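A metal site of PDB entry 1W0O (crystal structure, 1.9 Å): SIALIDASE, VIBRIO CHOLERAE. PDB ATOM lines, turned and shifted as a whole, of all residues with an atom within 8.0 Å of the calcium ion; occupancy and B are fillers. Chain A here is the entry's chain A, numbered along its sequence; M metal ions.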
ATOM      1  N   VAL A 246      11.695  17.580  -3.831  1.00  0.00           N
ATOM      2  CA  VAL A 246      12.997  17.124  -3.372  1.00  0.00           C
ATOM      3  C   VAL A 246      13.223  15.741  -3.975  1.00  0.00           C
ATOM      4  O   VAL A 246      12.568  14.769  -3.586  1.00  0.00           O
ATOM      5  CB  VAL A 246      13.056  17.030  -1.839  1.00  0.00           C
ATOM      6  CG1 VAL A 246      14.396  16.445  -1.399  1.00  0.00           C
ATOM      7  CG2 VAL A 246      12.841  18.402  -1.221  1.00  0.00           C
ATOM      8  N   GLY A 248      12.982  15.493  -7.216  1.00  0.00           N
ATOM      9  CA  GLY A 248      12.350  15.723  -8.508  1.00  0.00           C
ATOM     10  C   GLY A 248      11.272  14.722  -8.890  1.00  0.00           C
ATOM     11  O   GLY A 248      11.113  13.682  -8.248  1.00  0.00           O
ATOM     12  N   GLY A 249      10.515  15.048  -9.940  1.00  0.00           N
ATOM     13  CA  GLY A 249       9.486  14.150 -10.425  1.00  0.00           C
ATOM     14  C   GLY A 249       8.086  14.297  -9.848  1.00  0.00           C
ATOM     15  O   GLY A 249       7.874  14.974  -8.840  1.00  0.00           O
ATOM     16  N   ASP A 250       7.133  13.641 -10.509  1.00  0.00           N
ATOM     17  CA  ASP A 250       5.738  13.691 -10.095  1.00  0.00           C
ATOM     18  C   ASP A 250       5.527  13.010  -8.751  1.00  0.00           C
ATOM     19  O   ASP A 250       6.321  12.169  -8.336  1.00  0.00           O
ATOM     20  CB  ASP A 250       4.842  12.992 -11.126  1.00  0.00           C
ATOM     21  CG  ASP A 250       4.798  13.724 -12.451  1.00  0.00           C
ATOM     22  OD1 ASP A 250       5.316  14.861 -12.545  1.00  0.00           O
ATOM     23  OD2 ASP A 250       4.230  13.163 -13.412  1.00  0.00           O
ATOM     24  N   PRO A 251       4.441  13.364  -8.051  1.00  0.00           N
ATOM     25  CA  PRO A 251       4.167  12.759  -6.749  1.00  0.00           C
ATOM     26  C   PRO A 251       3.955  11.249  -6.893  1.00  0.00           C
ATOM     27  O   PRO A 251       3.587  10.765  -7.964  1.00  0.00           O
ATOM     28  CB  PRO A 251       2.901  13.479  -6.291  1.00  0.00           C
ATOM     29  CG  PRO A 251       2.211  13.814  -7.573  1.00  0.00           C
ATOM     30  CD  PRO A 251       3.353  14.286  -8.438  1.00  0.00           C
ATOM     31  N   GLY A 252       4.210  10.513  -5.808  1.00  0.00           N
ATOM     32  CA  GLY A 252       4.028   9.071  -5.827  1.00  0.00           C
ATOM     33  C   GLY A 252       5.328   8.280  -5.939  1.00  0.00           C
ATOM     34  O   GLY A 252       5.320   7.055  -5.866  1.00  0.00           O
ATOM     35  N   ALA A 253       6.446   8.979  -6.125  1.00  0.00           N
ATOM     36  CA  ALA A 253       7.730   8.306  -6.266  1.00  0.00           C
ATOM     37  C   ALA A 253       8.445   8.118  -4.937  1.00  0.00           C
ATOM     38  O   ALA A 253       8.471   9.029  -4.106  1.00  0.00           O
ATOM     39  CB  ALA A 253       8.631   9.079  -7.222  1.00  0.00           C
ATOM     40  N   LEU A 254       9.031   6.942  -4.734  1.00  0.00           N
ATOM     41  CA  LEU A 254       9.764   6.659  -3.504  1.00  0.00           C
ATOM     42  C   LEU A 254      10.989   7.552  -3.412  1.00  0.00           C
ATOM     43  O   LEU A 254      11.443   7.887  -2.313  1.00  0.00           O
ATOM     44  CB  LEU A 254      10.206   5.192  -3.487  1.00  0.00           C
ATOM     45  CG  LEU A 254       9.220   4.184  -2.923  1.00  0.00           C
ATOM     46  CD1 LEU A 254       9.700   2.763  -3.200  1.00  0.00           C
ATOM     47  CD2 LEU A 254       9.069   4.432  -1.420  1.00  0.00           C
ATOM     48  N   SER A 255      11.516   7.943  -4.567  1.00  0.00           N
ATOM     49  CA  SER A 255      12.712   8.785  -4.625  1.00  0.00           C
ATOM     50  C   SER A 255      12.491  10.272  -4.354  1.00  0.00           C
ATOM     51  O   SER A 255      13.449  11.039  -4.357  1.00  0.00           O
ATOM     52  CB  SER A 255      13.405   8.618  -5.984  1.00  0.00           C
ATOM     53  OG  SER A 255      12.524   8.975  -7.041  1.00  0.00           O
ATOM     54  N   ASN A 256      11.251  10.683  -4.126  1.00  0.00           N
ATOM     55  CA  ASN A 256      11.019  12.094  -3.833  1.00  0.00           C
ATOM     56  C   ASN A 256      10.081  12.358  -2.667  1.00  0.00           C
ATOM     57  O   ASN A 256       9.314  11.499  -2.254  1.00  0.00           O
ATOM     58  CB  ASN A 256      10.519  12.849  -5.081  1.00  0.00           C
ATOM     59  CG  ASN A 256       9.133  12.405  -5.537  1.00  0.00           C
ATOM     60  OD1 ASN A 256       8.334  11.869  -4.765  1.00  0.00           O
ATOM     61  ND2 ASN A 256       8.833  12.646  -6.815  1.00  0.00           N
ATOM     62  N   THR A 257      10.186  13.572  -2.127  1.00  0.00           N
ATOM     63  CA  THR A 257       9.327  14.020  -1.050  1.00  0.00           C
ATOM     64  C   THR A 257       8.870  15.396  -1.533  1.00  0.00           C
ATOM     65  O   THR A 257       9.655  16.344  -1.547  1.00  0.00           O
ATOM     66  CB  THR A 257      10.090  14.176   0.292  1.00  0.00           C
ATOM     67  OG1 THR A 257      10.645  12.917   0.681  1.00  0.00           O
ATOM     68  CG2 THR A 257       9.126  14.648   1.381  1.00  0.00           C
ATOM     69  N   ASN A 258       7.623  15.489  -1.978  1.00  0.00           N
ATOM     70  CA  ASN A 258       7.115  16.753  -2.509  1.00  0.00           C
ATOM     71  C   ASN A 258       6.238  17.522  -1.531  1.00  0.00           C
ATOM     72  O   ASN A 258       5.464  16.944  -0.782  1.00  0.00           O
ATOM     73  CB  ASN A 258       6.352  16.510  -3.813  1.00  0.00           C
ATOM     74  CG  ASN A 258       7.204  15.803  -4.855  1.00  0.00           C
ATOM     75  OD1 ASN A 258       8.413  15.661  -4.697  1.00  0.00           O
ATOM     76  ND2 ASN A 258       6.561  15.363  -5.943  1.00  0.00           N
ATOM     77  N   ASN A 283       3.950  16.912   7.248  1.00  0.00           N
ATOM     78  CA  ASN A 283       4.708  15.871   6.540  1.00  0.00           C
ATOM     79  C   ASN A 283       6.021  15.697   7.318  1.00  0.00           C
ATOM     80  O   ASN A 283       7.107  15.600   6.735  1.00  0.00           O
ATOM     81  CB  ASN A 283       4.984  16.337   5.104  1.00  0.00           C
ATOM     82  CG  ASN A 283       5.348  15.183   4.163  1.00  0.00           C
ATOM     83  OD1 ASN A 283       5.194  14.005   4.500  1.00  0.00           O
ATOM     84  ND2 ASN A 283       5.805  15.530   2.966  1.00  0.00           N
ATOM     85  N   ASP A 286       8.206  12.771   6.192  1.00  0.00           N
ATOM     86  CA  ASP A 286       8.345  12.638   4.751  1.00  0.00           C
ATOM     87  C   ASP A 286       7.549  11.441   4.250  1.00  0.00           C
ATOM     88  O   ASP A 286       7.942  10.770   3.302  1.00  0.00           O
ATOM     89  CB  ASP A 286       9.818  12.467   4.353  1.00  0.00           C
ATOM     90  CG  ASP A 286      10.659  13.685   4.669  1.00  0.00           C
ATOM     91  OD1 ASP A 286      10.088  14.801   4.720  1.00  0.00           O
ATOM     92  OD2 ASP A 286      11.883  13.541   4.853  1.00  0.00           O
ATOM     93  N   GLU A 287       6.405  11.187   4.891  1.00  0.00           N
ATOM     94  CA  GLU A 287       5.563  10.056   4.509  1.00  0.00           C
ATOM     95  C   GLU A 287       4.586  10.384   3.368  1.00  0.00           C
ATOM     96  O   GLU A 287       3.919   9.498   2.845  1.00  0.00           O
ATOM     97  CB  GLU A 287       4.755   9.557   5.716  1.00  0.00           C
ATOM     98  CG  GLU A 287       5.631   9.092   6.880  1.00  0.00           C
ATOM     99  CD  GLU A 287       4.844   8.400   7.963  1.00  0.00           C
ATOM    100  OE1 GLU A 287       3.804   8.948   8.404  1.00  0.00           O
ATOM    101  OE2 GLU A 287       5.267   7.304   8.409  1.00  0.00           O
ATOM    102  N   PHE A 288       4.521  11.653   2.999  1.00  0.00           N
ATOM    103  CA  PHE A 288       3.606  12.089   1.945  1.00  0.00           C
ATOM    104  C   PHE A 288       4.253  12.944   0.873  1.00  0.00           C
ATOM    105  O   PHE A 288       5.373  13.411   1.020  1.00  0.00           O
ATOM    106  CB  PHE A 288       2.480  12.948   2.519  1.00  0.00           C
ATOM    107  CG  PHE A 288       1.792  12.362   3.715  1.00  0.00           C
ATOM    108  CD1 PHE A 288       1.064  11.182   3.617  1.00  0.00           C
ATOM    109  CD2 PHE A 288       1.838  13.015   4.955  1.00  0.00           C
ATOM    110  CE1 PHE A 288       0.378  10.672   4.715  1.00  0.00           C
ATOM    111  CE2 PHE A 288       1.162  12.509   6.056  1.00  0.00           C
ATOM    112  CZ  PHE A 288       0.427  11.335   5.934  1.00  0.00           C
ATOM    113  N   ASP A 289       3.512  13.124  -0.212  1.00  0.00           N
ATOM    114  CA  ASP A 289       3.878  14.012  -1.299  1.00  0.00           C
ATOM    115  C   ASP A 289       2.635  14.891  -1.387  1.00  0.00           C
ATOM    116  O   ASP A 289       1.525  14.390  -1.232  1.00  0.00           O
ATOM    117  CB  ASP A 289       4.021  13.299  -2.651  1.00  0.00           C
ATOM    118  CG  ASP A 289       5.302  12.509  -2.776  1.00  0.00           C
ATOM    119  OD1 ASP A 289       6.331  12.924  -2.209  1.00  0.00           O
ATOM    120  OD2 ASP A 289       5.274  11.475  -3.487  1.00  0.00           O
ATOM    121  N   PHE A 290       2.819  16.191  -1.599  1.00  0.00           N
ATOM    122  CA  PHE A 290       1.671  17.077  -1.771  1.00  0.00           C
ATOM    123  C   PHE A 290       1.833  17.631  -3.179  1.00  0.00           C
ATOM    124  O   PHE A 290       2.956  17.776  -3.666  1.00  0.00           O
ATOM    125  CB  PHE A 290       1.677  18.215  -0.728  1.00  0.00           C
ATOM    126  CG  PHE A 290       1.336  17.747   0.667  1.00  0.00           C
ATOM    127  CD1 PHE A 290       2.314  17.211   1.498  1.00  0.00           C
ATOM    128  CD2 PHE A 290       0.020  17.798   1.118  1.00  0.00           C
ATOM    129  CE1 PHE A 290       1.992  16.726   2.761  1.00  0.00           C
ATOM    130  CE2 PHE A 290      -0.324  17.311   2.382  1.00  0.00           C
ATOM    131  CZ  PHE A 290       0.667  16.773   3.209  1.00  0.00           C
ATOM    132  N   TRP A 311      -0.747  12.764  -0.909  1.00  0.00           N
ATOM    133  CA  TRP A 311      -0.597  11.412  -1.430  1.00  0.00           C
ATOM    134  C   TRP A 311       0.413  10.673  -0.580  1.00  0.00           C
ATOM    135  O   TRP A 311       1.303  11.290   0.012  1.00  0.00           O
ATOM    136  CB  TRP A 311      -0.008  11.388  -2.854  1.00  0.00           C
ATOM    137  CG  TRP A 311      -0.579  12.339  -3.843  1.00  0.00           C
ATOM    138  CD1 TRP A 311      -0.186  13.628  -4.050  1.00  0.00           C
ATOM    139  CD2 TRP A 311      -1.657  12.080  -4.747  1.00  0.00           C
ATOM    140  NE1 TRP A 311      -0.962  14.197  -5.042  1.00  0.00           N
ATOM    141  CE2 TRP A 311      -1.869  13.272  -5.482  1.00  0.00           C
ATOM    142  CE3 TRP A 311      -2.456  10.970  -5.017  1.00  0.00           C
ATOM    143  CZ2 TRP A 311      -2.852  13.375  -6.470  1.00  0.00           C
ATOM    144  CZ3 TRP A 311      -3.442  11.070  -5.991  1.00  0.00           C
ATOM    145  CH2 TRP A 311      -3.632  12.271  -6.704  1.00  0.00           C
ATOM    146  N   PRO A 312       0.280   9.340  -0.478  1.00  0.00           N
ATOM    147  CA  PRO A 312       1.308   8.680   0.323  1.00  0.00           C
ATOM    148  C   PRO A 312       2.527   8.918  -0.582  1.00  0.00           C
ATOM    149  O   PRO A 312       2.362   9.029  -1.800  1.00  0.00           O
ATOM    150  CB  PRO A 312       0.856   7.220   0.351  1.00  0.00           C
ATOM    151  CG  PRO A 312       0.049   7.088  -0.924  1.00  0.00           C
ATOM    152  CD  PRO A 312      -0.724   8.375  -0.953  1.00  0.00           C
ATOM    153  N   THR A 313       3.731   9.024  -0.019  1.00  0.00           N
ATOM    154  CA  THR A 313       4.905   9.308  -0.847  1.00  0.00           C
ATOM    155  C   THR A 313       5.254   8.269  -1.915  1.00  0.00           C
ATOM    156  O   THR A 313       5.996   8.557  -2.848  1.00  0.00           O
ATOM    157  CB  THR A 313       6.163   9.545   0.022  1.00  0.00           C
ATOM    158  OG1 THR A 313       7.215  10.099  -0.780  1.00  0.00           O
ATOM    159  CG2 THR A 313       6.637   8.233   0.640  1.00  0.00           C
ATOM    160  N   ASP A 314       4.703   7.061  -1.775  1.00  0.00           N
ATOM    161  CA  ASP A 314       5.011   5.983  -2.711  1.00  0.00           C
ATOM    162  C   ASP A 314       3.907   5.531  -3.670  1.00  0.00           C
ATOM    163  O   ASP A 314       4.050   4.515  -4.338  1.00  0.00           O
ATOM    164  CB  ASP A 314       5.533   4.775  -1.929  1.00  0.00           C
ATOM    165  CG  ASP A 314       4.518   4.229  -0.952  1.00  0.00           C
ATOM    166  OD1 ASP A 314       3.524   4.936  -0.672  1.00  0.00           O
ATOM    167  OD2 ASP A 314       4.698   3.103  -0.459  1.00  0.00           O
ATOM    168  N   ALA A 315       2.810   6.295  -3.744  1.00  0.00           N
ATOM    169  CA  ALA A 315       1.707   5.964  -4.653  1.00  0.00           C
ATOM    170  C   ALA A 315       0.868   7.205  -4.960  1.00  0.00           C
ATOM    171  O   ALA A 315       0.447   7.920  -4.050  1.00  0.00           O
ATOM    172  CB  ALA A 315       0.833   4.864  -4.042  1.00  0.00           C
ATOM    173  N   ALA A 316       0.613   7.450  -6.241  1.00  0.00           N
ATOM    174  CA  ALA A 316      -0.177   8.608  -6.623  1.00  0.00           C
ATOM    175  C   ALA A 316      -1.049   8.376  -7.852  1.00  0.00           C
ATOM    176  O   ALA A 316      -1.373   7.243  -8.186  1.00  0.00           O
ATOM    177  CB  ALA A 316       0.738   9.830  -6.845  1.00  0.00           C
HETATM  178 CA    CA M   1       7.340  10.680  -3.057  1.00  0.00          CA
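Along chain A the residues within 4 Å of the calcium ion span positions 253 to 313.
The nearest printed residue that does not touch the calcium ion is Thr 257 (4.2 Å).
N of Thr 313 lies within hydrogen-bond range of O of Glu 287.
The side-chain carboxylate (OD2) of Asp 289 sits close to the backbone NH (N) of Gly 252 (2.7 Å).
The backbone carbonyl oxygen of Asp 250 is in hydrogen-bond range of the side-chain amide nitrogen of Asn 256, at 3.0 Å.
The backbone carbonyl oxygen of Asp 289 sits at hydrogen-bond distance from the backbone NH of Trp 311, 2.8 Å away.
The side-chain amide nitrogen of Asn 256 lies within hydrogen-bond range of the backbone carbonyl oxygen of Gly 248.
The side-chain carboxylate of Asp 289 sits close to the backbone NH of Asn 258, at 2.9 Å.
The side-chain amide nitrogen of Asn 256 sits at hydrogen-bond distance from the backbone carbonyl oxygen of Gly 249 (3.2 Å).
The calcium ion is bound by the side-chain carboxylate (OD2) of Asp 289 (2.3 Å), the backbone carbonyl oxygen (O) of Ala 253 (2.3 Å), the backbone carbonyl oxygen (O) of Asn 256 (2.3 Å), the side-chain amide oxygen (OD1) of Asn 256 (2.3 Å), the side-chain hydroxyl (OG1) of Thr 313 (2.4 Å), the backbone carbonyl oxygen (O) of Thr 313 (2.5 Å) and the side-chain carboxylate (OD1) of Asp 289 (2.6 Å).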
